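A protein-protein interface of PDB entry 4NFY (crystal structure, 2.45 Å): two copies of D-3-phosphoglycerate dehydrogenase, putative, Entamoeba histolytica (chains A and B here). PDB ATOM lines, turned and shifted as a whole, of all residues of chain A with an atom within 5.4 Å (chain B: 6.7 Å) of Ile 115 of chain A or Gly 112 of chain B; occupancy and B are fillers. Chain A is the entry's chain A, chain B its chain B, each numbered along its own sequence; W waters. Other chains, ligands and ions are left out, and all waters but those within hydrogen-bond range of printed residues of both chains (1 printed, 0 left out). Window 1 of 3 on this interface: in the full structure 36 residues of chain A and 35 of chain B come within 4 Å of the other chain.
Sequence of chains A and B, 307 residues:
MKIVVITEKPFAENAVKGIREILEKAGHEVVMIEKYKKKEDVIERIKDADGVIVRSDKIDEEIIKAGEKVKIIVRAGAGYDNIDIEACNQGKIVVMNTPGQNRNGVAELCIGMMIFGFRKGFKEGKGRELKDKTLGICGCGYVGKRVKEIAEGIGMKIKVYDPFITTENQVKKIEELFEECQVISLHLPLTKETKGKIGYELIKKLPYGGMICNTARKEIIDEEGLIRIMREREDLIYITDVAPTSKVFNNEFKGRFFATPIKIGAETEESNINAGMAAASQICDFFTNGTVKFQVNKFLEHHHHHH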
ATOM      1  N   CYS A 110      14.058  -9.129   0.421  1.00  0.00           N
ATOM      2  CA  CYS A 110      15.045 -10.055   0.986  1.00  0.00           C
ATOM      3  C   CYS A 110      16.221 -10.228   0.022  1.00  0.00           C
ATOM      4  O   CYS A 110      17.378 -10.134   0.425  1.00  0.00           O
ATOM      5  CB  CYS A 110      14.389 -11.403   1.335  1.00  0.00           C
ATOM      6  SG  CYS A 110      15.531 -12.697   1.859  1.00  0.00           S
ATOM      7  N   ILE A 111      15.920 -10.417  -1.258  1.00  0.00           N
ATOM      8  CA  ILE A 111      16.958 -10.628  -2.271  1.00  0.00           C
ATOM      9  C   ILE A 111      17.800  -9.374  -2.455  1.00  0.00           C
ATOM     10  O   ILE A 111      19.023  -9.444  -2.582  1.00  0.00           O
ATOM     11  CB  ILE A 111      16.354 -11.065  -3.634  1.00  0.00           C
ATOM     12  CG1 ILE A 111      15.628 -12.415  -3.515  1.00  0.00           C
ATOM     13  CG2 ILE A 111      17.429 -11.157  -4.705  1.00  0.00           C
ATOM     14  CD1 ILE A 111      16.546 -13.626  -3.398  1.00  0.00           C
ATOM     15  N   GLY A 112      17.144  -8.226  -2.483  1.00  0.00           N
ATOM     16  CA  GLY A 112      17.844  -6.955  -2.597  1.00  0.00           C
ATOM     17  C   GLY A 112      18.788  -6.732  -1.437  1.00  0.00           C
ATOM     18  O   GLY A 112      19.888  -6.228  -1.607  1.00  0.00           O
ATOM     19  N   MET A 113      18.350  -7.118  -0.255  1.00  0.00           N
ATOM     20  CA  MET A 113      19.142  -6.931   0.945  1.00  0.00           C
ATOM     21  C   MET A 113      20.321  -7.862   0.990  1.00  0.00           C
ATOM     22  O   MET A 113      21.389  -7.502   1.509  1.00  0.00           O
ATOM     23  CB  MET A 113      18.284  -7.150   2.177  1.00  0.00           C
ATOM     24  CG  MET A 113      17.494  -5.914   2.555  1.00  0.00           C
ATOM     25  SD  MET A 113      16.506  -6.230   4.007  1.00  0.00           S
ATOM     26  CE  MET A 113      16.150  -4.531   4.434  1.00  0.00           C
ATOM     27  N   MET A 114      20.127  -9.061   0.453  1.00  0.00           N
ATOM     28  CA  MET A 114      21.199 -10.018   0.393  1.00  0.00           C
ATOM     29  C   MET A 114      22.293  -9.529  -0.530  1.00  0.00           C
ATOM     30  O   MET A 114      23.481  -9.616  -0.198  1.00  0.00           O
ATOM     31  CB  MET A 114      20.677 -11.382  -0.049  1.00  0.00           C
ATOM     32  CG  MET A 114      19.935 -12.063   1.077  1.00  0.00           C
ATOM     33  SD  MET A 114      19.383 -13.705   0.667  1.00  0.00           S
ATOM     34  CE  MET A 114      18.175 -13.391  -0.597  1.00  0.00           C
ATOM     35  N   ILE A 115      21.900  -8.997  -1.678  1.00  0.00           N
ATOM     36  CA  ILE A 115      22.882  -8.459  -2.608  1.00  0.00           C
ATOM     37  C   ILE A 115      23.561  -7.249  -1.963  1.00  0.00           C
ATOM     38  O   ILE A 115      24.776  -7.125  -2.014  1.00  0.00           O
ATOM     39  CB  ILE A 115      22.259  -8.073  -3.960  1.00  0.00           C
ATOM     40  CG1 ILE A 115      21.681  -9.301  -4.643  1.00  0.00           C
ATOM     41  CG2 ILE A 115      23.304  -7.415  -4.855  1.00  0.00           C
ATOM     42  CD1 ILE A 115      20.900  -8.970  -5.893  1.00  0.00           C
ATOM     43  N   PHE A 116      22.762  -6.393  -1.332  1.00  0.00           N
ATOM     44  CA  PHE A 116      23.253  -5.220  -0.606  1.00  0.00           C
ATOM     45  C   PHE A 116      24.310  -5.607   0.431  1.00  0.00           C
ATOM     46  O   PHE A 116      25.429  -5.096   0.410  1.00  0.00           O
ATOM     47  CB  PHE A 116      22.069  -4.528   0.052  1.00  0.00           C
ATOM     48  CG  PHE A 116      22.373  -3.184   0.648  1.00  0.00           C
ATOM     49  CD1 PHE A 116      22.448  -2.060  -0.149  1.00  0.00           C
ATOM     50  CD2 PHE A 116      22.492  -3.032   2.016  1.00  0.00           C
ATOM     51  CE1 PHE A 116      22.677  -0.810   0.404  1.00  0.00           C
ATOM     52  CE2 PHE A 116      22.732  -1.794   2.573  1.00  0.00           C
ATOM     53  CZ  PHE A 116      22.820  -0.679   1.767  1.00  0.00           C
ATOM     54  N   GLY A 117      23.982  -6.546   1.304  1.00  0.00           N
ATOM     55  CA  GLY A 117      24.932  -6.991   2.337  1.00  0.00           C
ATOM     56  C   GLY A 117      26.195  -7.606   1.758  1.00  0.00           C
ATOM     57  O   GLY A 117      27.302  -7.297   2.197  1.00  0.00           O
ATOM     58  N   PHE A 118      26.037  -8.459   0.751  1.00  0.00           N
ATOM     59  CA  PHE A 118      27.189  -9.066   0.048  1.00  0.00           C
ATOM     60  C   PHE A 118      28.066  -8.044  -0.678  1.00  0.00           C
ATOM     61  O   PHE A 118      29.197  -8.363  -1.052  1.00  0.00           O
ATOM     62  CB  PHE A 118      26.713 -10.147  -0.953  1.00  0.00           C
ATOM     63  CG  PHE A 118      26.932 -11.585  -0.499  1.00  0.00           C
ATOM     64  CD1 PHE A 118      27.255 -11.913   0.824  1.00  0.00           C
ATOM     65  CD2 PHE A 118      26.787 -12.632  -1.419  1.00  0.00           C
ATOM     66  CE1 PHE A 118      27.455 -13.233   1.203  1.00  0.00           C
ATOM     67  CE2 PHE A 118      26.981 -13.951  -1.035  1.00  0.00           C
ATOM     68  CZ  PHE A 118      27.318 -14.252   0.282  1.00  0.00           C
ATOM     69  N   ARG A 119      27.551  -6.830  -0.869  1.00  0.00           N
ATOM     70  CA  ARG A 119      28.264  -5.764  -1.549  1.00  0.00           C
ATOM     71  C   ARG A 119      28.495  -4.523  -0.675  1.00  0.00           C
ATOM     72  O   ARG A 119      28.611  -3.391  -1.176  1.00  0.00           O
ATOM     73  CB  ARG A 119      27.464  -5.385  -2.779  1.00  0.00           C
ATOM     74  CG  ARG A 119      27.355  -6.520  -3.753  1.00  0.00           C
ATOM     75  CD  ARG A 119      28.707  -6.805  -4.385  1.00  0.00           C
ATOM     76  NE  ARG A 119      28.423  -7.543  -5.582  1.00  0.00           N
ATOM     77  CZ  ARG A 119      28.675  -7.164  -6.822  1.00  0.00           C
ATOM     78  NH1 ARG A 119      29.362  -6.080  -7.120  1.00  0.00           N
ATOM     79  NH2 ARG A 119      28.270  -7.956  -7.778  1.00  0.00           N
ATOM     80  N   LYS A 120      28.558  -4.741   0.630  1.00  0.00           N
ATOM     81  CA  LYS A 120      29.013  -3.737   1.561  1.00  0.00           C
ATOM     82  C   LYS A 120      28.192  -2.458   1.510  1.00  0.00           C
ATOM     83  O   LYS A 120      28.725  -1.367   1.659  1.00  0.00           O
ATOM     84  CB  LYS A 120      30.483  -3.426   1.296  1.00  0.00           C
ATOM     85  CG  LYS A 120      31.328  -4.647   0.986  1.00  0.00           C
ATOM     86  CD  LYS A 120      32.802  -4.319   1.128  1.00  0.00           C
ATOM     87  CE  LYS A 120      33.324  -4.642   2.521  1.00  0.00           C
ATOM     88  NZ  LYS A 120      33.654  -6.089   2.630  1.00  0.00           N
ATOM     89  N   PHE A 122      26.758  -1.193  -1.071  1.00  0.00           N
ATOM     90  CA  PHE A 122      27.121  -0.471  -2.288  1.00  0.00           C
ATOM     91  C   PHE A 122      28.179   0.604  -2.012  1.00  0.00           C
ATOM     92  O   PHE A 122      28.144   1.707  -2.569  1.00  0.00           O
ATOM     93  CB  PHE A 122      25.878   0.114  -2.993  1.00  0.00           C
ATOM     94  CG  PHE A 122      24.809  -0.904  -3.314  1.00  0.00           C
ATOM     95  CD1 PHE A 122      25.120  -2.239  -3.545  1.00  0.00           C
ATOM     96  CD2 PHE A 122      23.477  -0.514  -3.412  1.00  0.00           C
ATOM     97  CE1 PHE A 122      24.126  -3.160  -3.842  1.00  0.00           C
ATOM     98  CE2 PHE A 122      22.481  -1.437  -3.707  1.00  0.00           C
ATOM     99  CZ  PHE A 122      22.809  -2.763  -3.918  1.00  0.00           C
ATOM    100  N   LEU A 130      25.744 -13.943  -5.053  1.00  0.00           N
ATOM    101  CA  LEU A 130      24.779 -14.936  -4.603  1.00  0.00           C
ATOM    102  C   LEU A 130      24.786 -16.193  -5.483  1.00  0.00           C
ATOM    103  O   LEU A 130      24.554 -17.305  -5.002  1.00  0.00           O
ATOM    104  CB  LEU A 130      23.385 -14.323  -4.562  1.00  0.00           C
ATOM    105  CG  LEU A 130      23.174 -13.140  -3.610  1.00  0.00           C
ATOM    106  CD1 LEU A 130      21.740 -12.644  -3.707  1.00  0.00           C
ATOM    107  CD2 LEU A 130      23.497 -13.510  -2.165  1.00  0.00           C
ATOM    108  N   ILE A 154      18.190 -16.518  -9.715  1.00  0.00           N
ATOM    109  CA  ILE A 154      19.484 -15.883  -9.765  1.00  0.00           C
ATOM    110  C   ILE A 154      20.620 -16.873  -9.498  1.00  0.00           C
ATOM    111  O   ILE A 154      21.766 -16.476  -9.387  1.00  0.00           O
ATOM    112  CB  ILE A 154      19.513 -14.658  -8.839  1.00  0.00           C
ATOM    113  CG1 ILE A 154      19.688 -15.034  -7.375  1.00  0.00           C
ATOM    114  CG2 ILE A 154      18.209 -13.892  -8.978  1.00  0.00           C
ATOM    115  CD1 ILE A 154      19.644 -13.840  -6.450  1.00  0.00           C
ATOM    116  N   MET A 211      26.023 -15.162   6.056  1.00  0.00           N
ATOM    117  CA  MET A 211      25.108 -14.029   6.044  1.00  0.00           C
ATOM    118  C   MET A 211      23.723 -14.472   6.467  1.00  0.00           C
ATOM    119  O   MET A 211      23.229 -15.520   6.055  1.00  0.00           O
ATOM    120  CB  MET A 211      25.049 -13.385   4.661  1.00  0.00           C
ATOM    121  CG  MET A 211      24.169 -12.148   4.596  1.00  0.00           C
ATOM    122  SD  MET A 211      24.284 -11.297   3.017  1.00  0.00           S
ATOM    123  CE  MET A 211      23.269  -9.905   3.338  1.00  0.00           C
ATOM    124  N   ALA B 107      26.159  -7.834 -13.166  1.00  0.00           N
ATOM    125  CA  ALA B 107      24.721  -8.146 -13.309  1.00  0.00           C
ATOM    126  C   ALA B 107      23.985  -8.197 -11.970  1.00  0.00           C
ATOM    127  O   ALA B 107      22.911  -7.638 -11.836  1.00  0.00           O
ATOM    128  CB  ALA B 107      24.526  -9.467 -14.045  1.00  0.00           C
ATOM    129  N   GLU B 108      24.562  -8.879 -10.985  1.00  0.00           N
ATOM    130  CA  GLU B 108      23.984  -8.899  -9.639  1.00  0.00           C
ATOM    131  C   GLU B 108      23.981  -7.519  -9.019  1.00  0.00           C
ATOM    132  O   GLU B 108      23.058  -7.155  -8.315  1.00  0.00           O
ATOM    133  CB  GLU B 108      24.713  -9.880  -8.714  1.00  0.00           C
ATOM    134  CG  GLU B 108      24.325 -11.338  -8.943  1.00  0.00           C
ATOM    135  CD  GLU B 108      24.868 -12.292  -7.879  1.00  0.00           C
ATOM    136  OE1 GLU B 108      25.343 -11.845  -6.813  1.00  0.00           O
ATOM    137  OE2 GLU B 108      24.817 -13.513  -8.100  1.00  0.00           O
ATOM    138  N   LEU B 109      25.002  -6.732  -9.275  1.00  0.00           N
ATOM    139  CA  LEU B 109      25.002  -5.377  -8.742  1.00  0.00           C
ATOM    140  C   LEU B 109      23.853  -4.596  -9.391  1.00  0.00           C
ATOM    141  O   LEU B 109      23.171  -3.827  -8.735  1.00  0.00           O
ATOM    142  CB  LEU B 109      26.350  -4.698  -8.978  1.00  0.00           C
ATOM    143  CG  LEU B 109      26.767  -3.489  -8.136  1.00  0.00           C
ATOM    144  CD1 LEU B 109      26.673  -2.199  -8.931  1.00  0.00           C
ATOM    145  CD2 LEU B 109      26.012  -3.368  -6.821  1.00  0.00           C
ATOM    146  N   CYS B 110      23.612  -4.843 -10.674  1.00  0.00           N
ATOM    147  CA  CYS B 110      22.561  -4.149 -11.394  1.00  0.00           C
ATOM    148  C   CYS B 110      21.177  -4.458 -10.817  1.00  0.00           C
ATOM    149  O   CYS B 110      20.386  -3.544 -10.561  1.00  0.00           O
ATOM    150  CB  CYS B 110      22.638  -4.505 -12.883  1.00  0.00           C
ATOM    151  SG  CYS B 110      21.285  -3.856 -13.881  1.00  0.00           S
ATOM    152  N   ILE B 111      20.892  -5.737 -10.581  1.00  0.00           N
ATOM    153  CA  ILE B 111      19.586  -6.148 -10.045  1.00  0.00           C
ATOM    154  C   ILE B 111      19.414  -5.640  -8.621  1.00  0.00           C
ATOM    155  O   ILE B 111      18.334  -5.205  -8.229  1.00  0.00           O
ATOM    156  CB  ILE B 111      19.419  -7.682 -10.028  1.00  0.00           C
ATOM    157  CG1 ILE B 111      19.471  -8.283 -11.441  1.00  0.00           C
ATOM    158  CG2 ILE B 111      18.110  -8.068  -9.364  1.00  0.00           C
ATOM    159  CD1 ILE B 111      18.227  -8.056 -12.282  1.00  0.00           C
ATOM    160  N   GLY B 112      20.480  -5.728  -7.842  1.00  0.00           N
ATOM    161  CA  GLY B 112      20.490  -5.205  -6.481  1.00  0.00           C
ATOM    162  C   GLY B 112      20.182  -3.728  -6.443  1.00  0.00           C
ATOM    163  O   GLY B 112      19.387  -3.282  -5.630  1.00  0.00           O
ATOM    164  N   MET B 113      20.808  -2.985  -7.341  1.00  0.00           N
ATOM    165  CA  MET B 113      20.583  -1.547  -7.468  1.00  0.00           C
ATOM    166  C   MET B 113      19.181  -1.225  -7.944  1.00  0.00           C
ATOM    167  O   MET B 113      18.612  -0.203  -7.564  1.00  0.00           O
ATOM    168  CB  MET B 113      21.584  -0.931  -8.439  1.00  0.00           C
ATOM    169  CG  MET B 113      22.905  -0.566  -7.797  1.00  0.00           C
ATOM    170  SD  MET B 113      24.042   0.081  -9.024  1.00  0.00           S
ATOM    171  CE  MET B 113      25.198   0.849  -7.899  1.00  0.00           C
ATOM    172  N   MET B 114      18.632  -2.088  -8.792  1.00  0.00           N
ATOM    173  CA  MET B 114      17.260  -1.924  -9.235  1.00  0.00           C
ATOM    174  C   MET B 114      16.267  -2.107  -8.106  1.00  0.00           C
ATOM    175  O   MET B 114      15.301  -1.347  -7.996  1.00  0.00           O
ATOM    176  CB  MET B 114      16.936  -2.903 -10.352  1.00  0.00           C
ATOM    177  CG  MET B 114      17.481  -2.475 -11.694  1.00  0.00           C
ATOM    178  SD  MET B 114      17.185  -3.785 -12.874  1.00  0.00           S
ATOM    179  CE  MET B 114      18.152  -3.187 -14.241  1.00  0.00           C
ATOM    180  N   ILE B 115      16.483  -3.122  -7.276  1.00  0.00           N
ATOM    181  CA  ILE B 115      15.593  -3.339  -6.134  1.00  0.00           C
ATOM    182  C   ILE B 115      15.759  -2.154  -5.180  1.00  0.00           C
ATOM    183  O   ILE B 115      14.783  -1.489  -4.848  1.00  0.00           O
ATOM    184  CB  ILE B 115      15.867  -4.688  -5.442  1.00  0.00           C
ATOM    185  CG1 ILE B 115      15.525  -5.837  -6.379  1.00  0.00           C
ATOM    186  CG2 ILE B 115      15.074  -4.819  -4.149  1.00  0.00           C
ATOM    187  CD1 ILE B 115      16.060  -7.172  -5.911  1.00  0.00           C
ATOM    188  N   PHE B 116      17.000  -1.867  -4.801  1.00  0.00           N
ATOM    189  CA  PHE B 116      17.353  -0.675  -4.020  1.00  0.00           C
ATOM    190  C   PHE B 116      16.630   0.591  -4.524  1.00  0.00           C
ATOM    191  O   PHE B 116      15.874   1.227  -3.790  1.00  0.00           O
ATOM    192  CB  PHE B 116      18.872  -0.492  -4.073  1.00  0.00           C
ATOM    193  CG  PHE B 116      19.429   0.488  -3.074  1.00  0.00           C
ATOM    194  CD1 PHE B 116      19.620   0.125  -1.755  1.00  0.00           C
ATOM    195  CD2 PHE B 116      19.833   1.750  -3.469  1.00  0.00           C
ATOM    196  CE1 PHE B 116      20.172   1.012  -0.835  1.00  0.00           C
ATOM    197  CE2 PHE B 116      20.378   2.636  -2.558  1.00  0.00           C
ATOM    198  CZ  PHE B 116      20.548   2.266  -1.237  1.00  0.00           C
ATOM    199  N   GLY B 117      16.839   0.946  -5.781  1.00  0.00           N
ATOM    200  CA  GLY B 117      16.161   2.103  -6.376  1.00  0.00           C
ATOM    201  C   GLY B 117      14.662   2.038  -6.180  1.00  0.00           C
ATOM    202  O   GLY B 117      14.057   3.005  -5.732  1.00  0.00           O
ATOM    203  N   PHE B 122      16.046   1.489   0.626  1.00  0.00           N
ATOM    204  CA  PHE B 122      15.730   0.765   1.850  1.00  0.00           C
ATOM    205  C   PHE B 122      15.334   1.710   2.986  1.00  0.00           C
ATOM    206  O   PHE B 122      15.552   1.413   4.153  1.00  0.00           O
ATOM    207  CB  PHE B 122      16.875  -0.178   2.276  1.00  0.00           C
ATOM    208  CG  PHE B 122      17.235  -1.230   1.258  1.00  0.00           C
ATOM    209  CD1 PHE B 122      16.346  -1.629   0.269  1.00  0.00           C
ATOM    210  CD2 PHE B 122      18.468  -1.868   1.326  1.00  0.00           C
ATOM    211  CE1 PHE B 122      16.692  -2.614  -0.648  1.00  0.00           C
ATOM    212  CE2 PHE B 122      18.819  -2.853   0.411  1.00  0.00           C
ATOM    213  CZ  PHE B 122      17.927  -3.224  -0.579  1.00  0.00           C
ATOM    214  N   LEU B 130       9.997  -5.396  -9.092  1.00  0.00           N
ATOM    215  CA  LEU B 130      10.501  -5.685 -10.423  1.00  0.00           C
ATOM    216  C   LEU B 130       9.661  -6.750 -11.138  1.00  0.00           C
ATOM    217  O   LEU B 130       9.526  -6.725 -12.362  1.00  0.00           O
ATOM    218  CB  LEU B 130      11.962  -6.121 -10.349  1.00  0.00           C
ATOM    219  CG  LEU B 130      12.947  -5.126  -9.724  1.00  0.00           C
ATOM    220  CD1 LEU B 130      14.331  -5.745  -9.680  1.00  0.00           C
ATOM    221  CD2 LEU B 130      12.980  -3.796 -10.477  1.00  0.00           C
ATOM    222  N   ILE B 150      19.008 -13.133 -15.028  1.00  0.00           N
ATOM    223  CA  ILE B 150      18.602 -12.859 -13.645  1.00  0.00           C
ATOM    224  C   ILE B 150      17.226 -12.192 -13.610  1.00  0.00           C
ATOM    225  O   ILE B 150      16.339 -12.594 -12.845  1.00  0.00           O
ATOM    226  CB  ILE B 150      19.618 -11.973 -12.888  1.00  0.00           C
ATOM    227  CG1 ILE B 150      21.009 -12.613 -12.880  1.00  0.00           C
ATOM    228  CG2 ILE B 150      19.146 -11.784 -11.457  1.00  0.00           C
ATOM    229  CD1 ILE B 150      22.064 -11.809 -12.145  1.00  0.00           C
ATOM    230  N   ILE B 239      19.915   5.137 -10.895  1.00  0.00           N
ATOM    231  CA  ILE B 239      20.858   4.424 -10.034  1.00  0.00           C
ATOM    232  C   ILE B 239      22.038   4.073 -10.901  1.00  0.00           C
ATOM    233  O   ILE B 239      21.850   3.580 -12.016  1.00  0.00           O
ATOM    234  CB  ILE B 239      20.291   3.096  -9.488  1.00  0.00           C
ATOM    235  CG1 ILE B 239      18.837   3.240  -9.065  1.00  0.00           C
ATOM    236  CG2 ILE B 239      21.135   2.604  -8.316  1.00  0.00           C
ATOM    237  CD1 ILE B 239      18.659   3.965  -7.750  1.00  0.00           C
HETATM  238  O   HOH W   1      26.500  -9.701  -5.599  1.00  0.00           O
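The backbone NH (N) of Leu 130 of chain A lies within hydrogen-bond range of the side-chain carboxylate (OE1) of Glu 108 of chain B (2.8 Å).
Among the printed residues, merely in contact across the chains: Phe 116 of chain A with Phe 116 of chain B (3.3 Å), Ile 154 of chain A with Ile 150 of chain B (3.4 Å), Ile 115 of chain A with Glu 108 of chain B (3.5 Å), Phe 122 of chain A with Leu 109 of chain B (3.5 Å), Phe 116 of chain A with Phe 122 of chain B (3.6 Å), Phe 122 of chain A with Phe 116 of chain B (3.7 Å), Gly 112 of chain A with Phe 122 of chain B (3.7 Å), Gly 112 of chain A with Ile 115 of chain B (3.7 Å), Phe 122 of chain A with Gly 112 of chain B (3.8 Å), Arg 119 of chain A with Leu 109 of chain B (3.8 Å), Ile 115 of chain A with Gly 112 of chain B (3.8 Å), Met 113 of chain A with Phe 122 of chain B (3.9 Å) and Phe 122 of chain A with Met 113 of chain B (3.97 Å).
Ile 115 of chain A touches just these residues of chain B: Glu 108 and Gly 112.
Of chain A, only Ile 115 and Phe 122 come within 4 Å of Gly 112 of chain B.
Of the printed residues of chain B, Met 113 of chain A touches Phe 122 (3.9 Å).
Of the printed residues of chain B, Gly 112 of chain A touches Ile 115 and Phe 122.
Printed residues of chain B within 4 Å of Phe 116 of chain A: Phe 116 and Phe 122.
The nearest residue of chain B that does not touch Ile 115 of chain A is Ile 111 of chain B (4.5 Å).
The nearest residue of chain A that does not touch Gly 112 of chain B is Gly 112 of chain A (5.0 Å).
Of the 15 printed residues of chain B, 8 touch a printed residue of chain A.
Hydrophobic or aromatic side chains of chain B that line the printed part of chain A: Leu 109, Ile 115, Phe 116, Phe 122 and Ile 150.
Hydrophobic or aromatic side chains of chain A that line the printed part of chain B: Met 113, Ile 115, Phe 116, Phe 122, Leu 130 and Ile 154.
Along chain A the printed residues that touch a printed residue of chain B span positions 112 to 154.
Gly 112 of chain A touches Ile 115 of chain B, and with the chains exchanged Ile 115 of chain A touches Gly 112 of chain B.
Gly 112 of chain A touches Phe 122 of chain B, and with the chains exchanged Phe 122 of chain A touches Gly 112 of chain B.
Met 113 of chain A touches Phe 122 of chain B, and with the chains exchanged Phe 122 of chain A touches Met 113 of chain B.
Phe 116 of chain A touches Phe 122 of chain B, and with the chains exchanged Phe 122 of chain A touches Phe 116 of chain B.
Positions printed for both chains: 110, 111, 112, 113, 114, 115, 116, 117, 122 and 130.
Of the 14 pairs that touch across the chains among the printed residues, 9 have their exchanged pair printed and touching as well.
Water W1 lies within hydrogen-bond range of OE1 of Glu 108 of chain B (2.7 Å) and NE of Arg 119 of chain A (2.9 Å).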
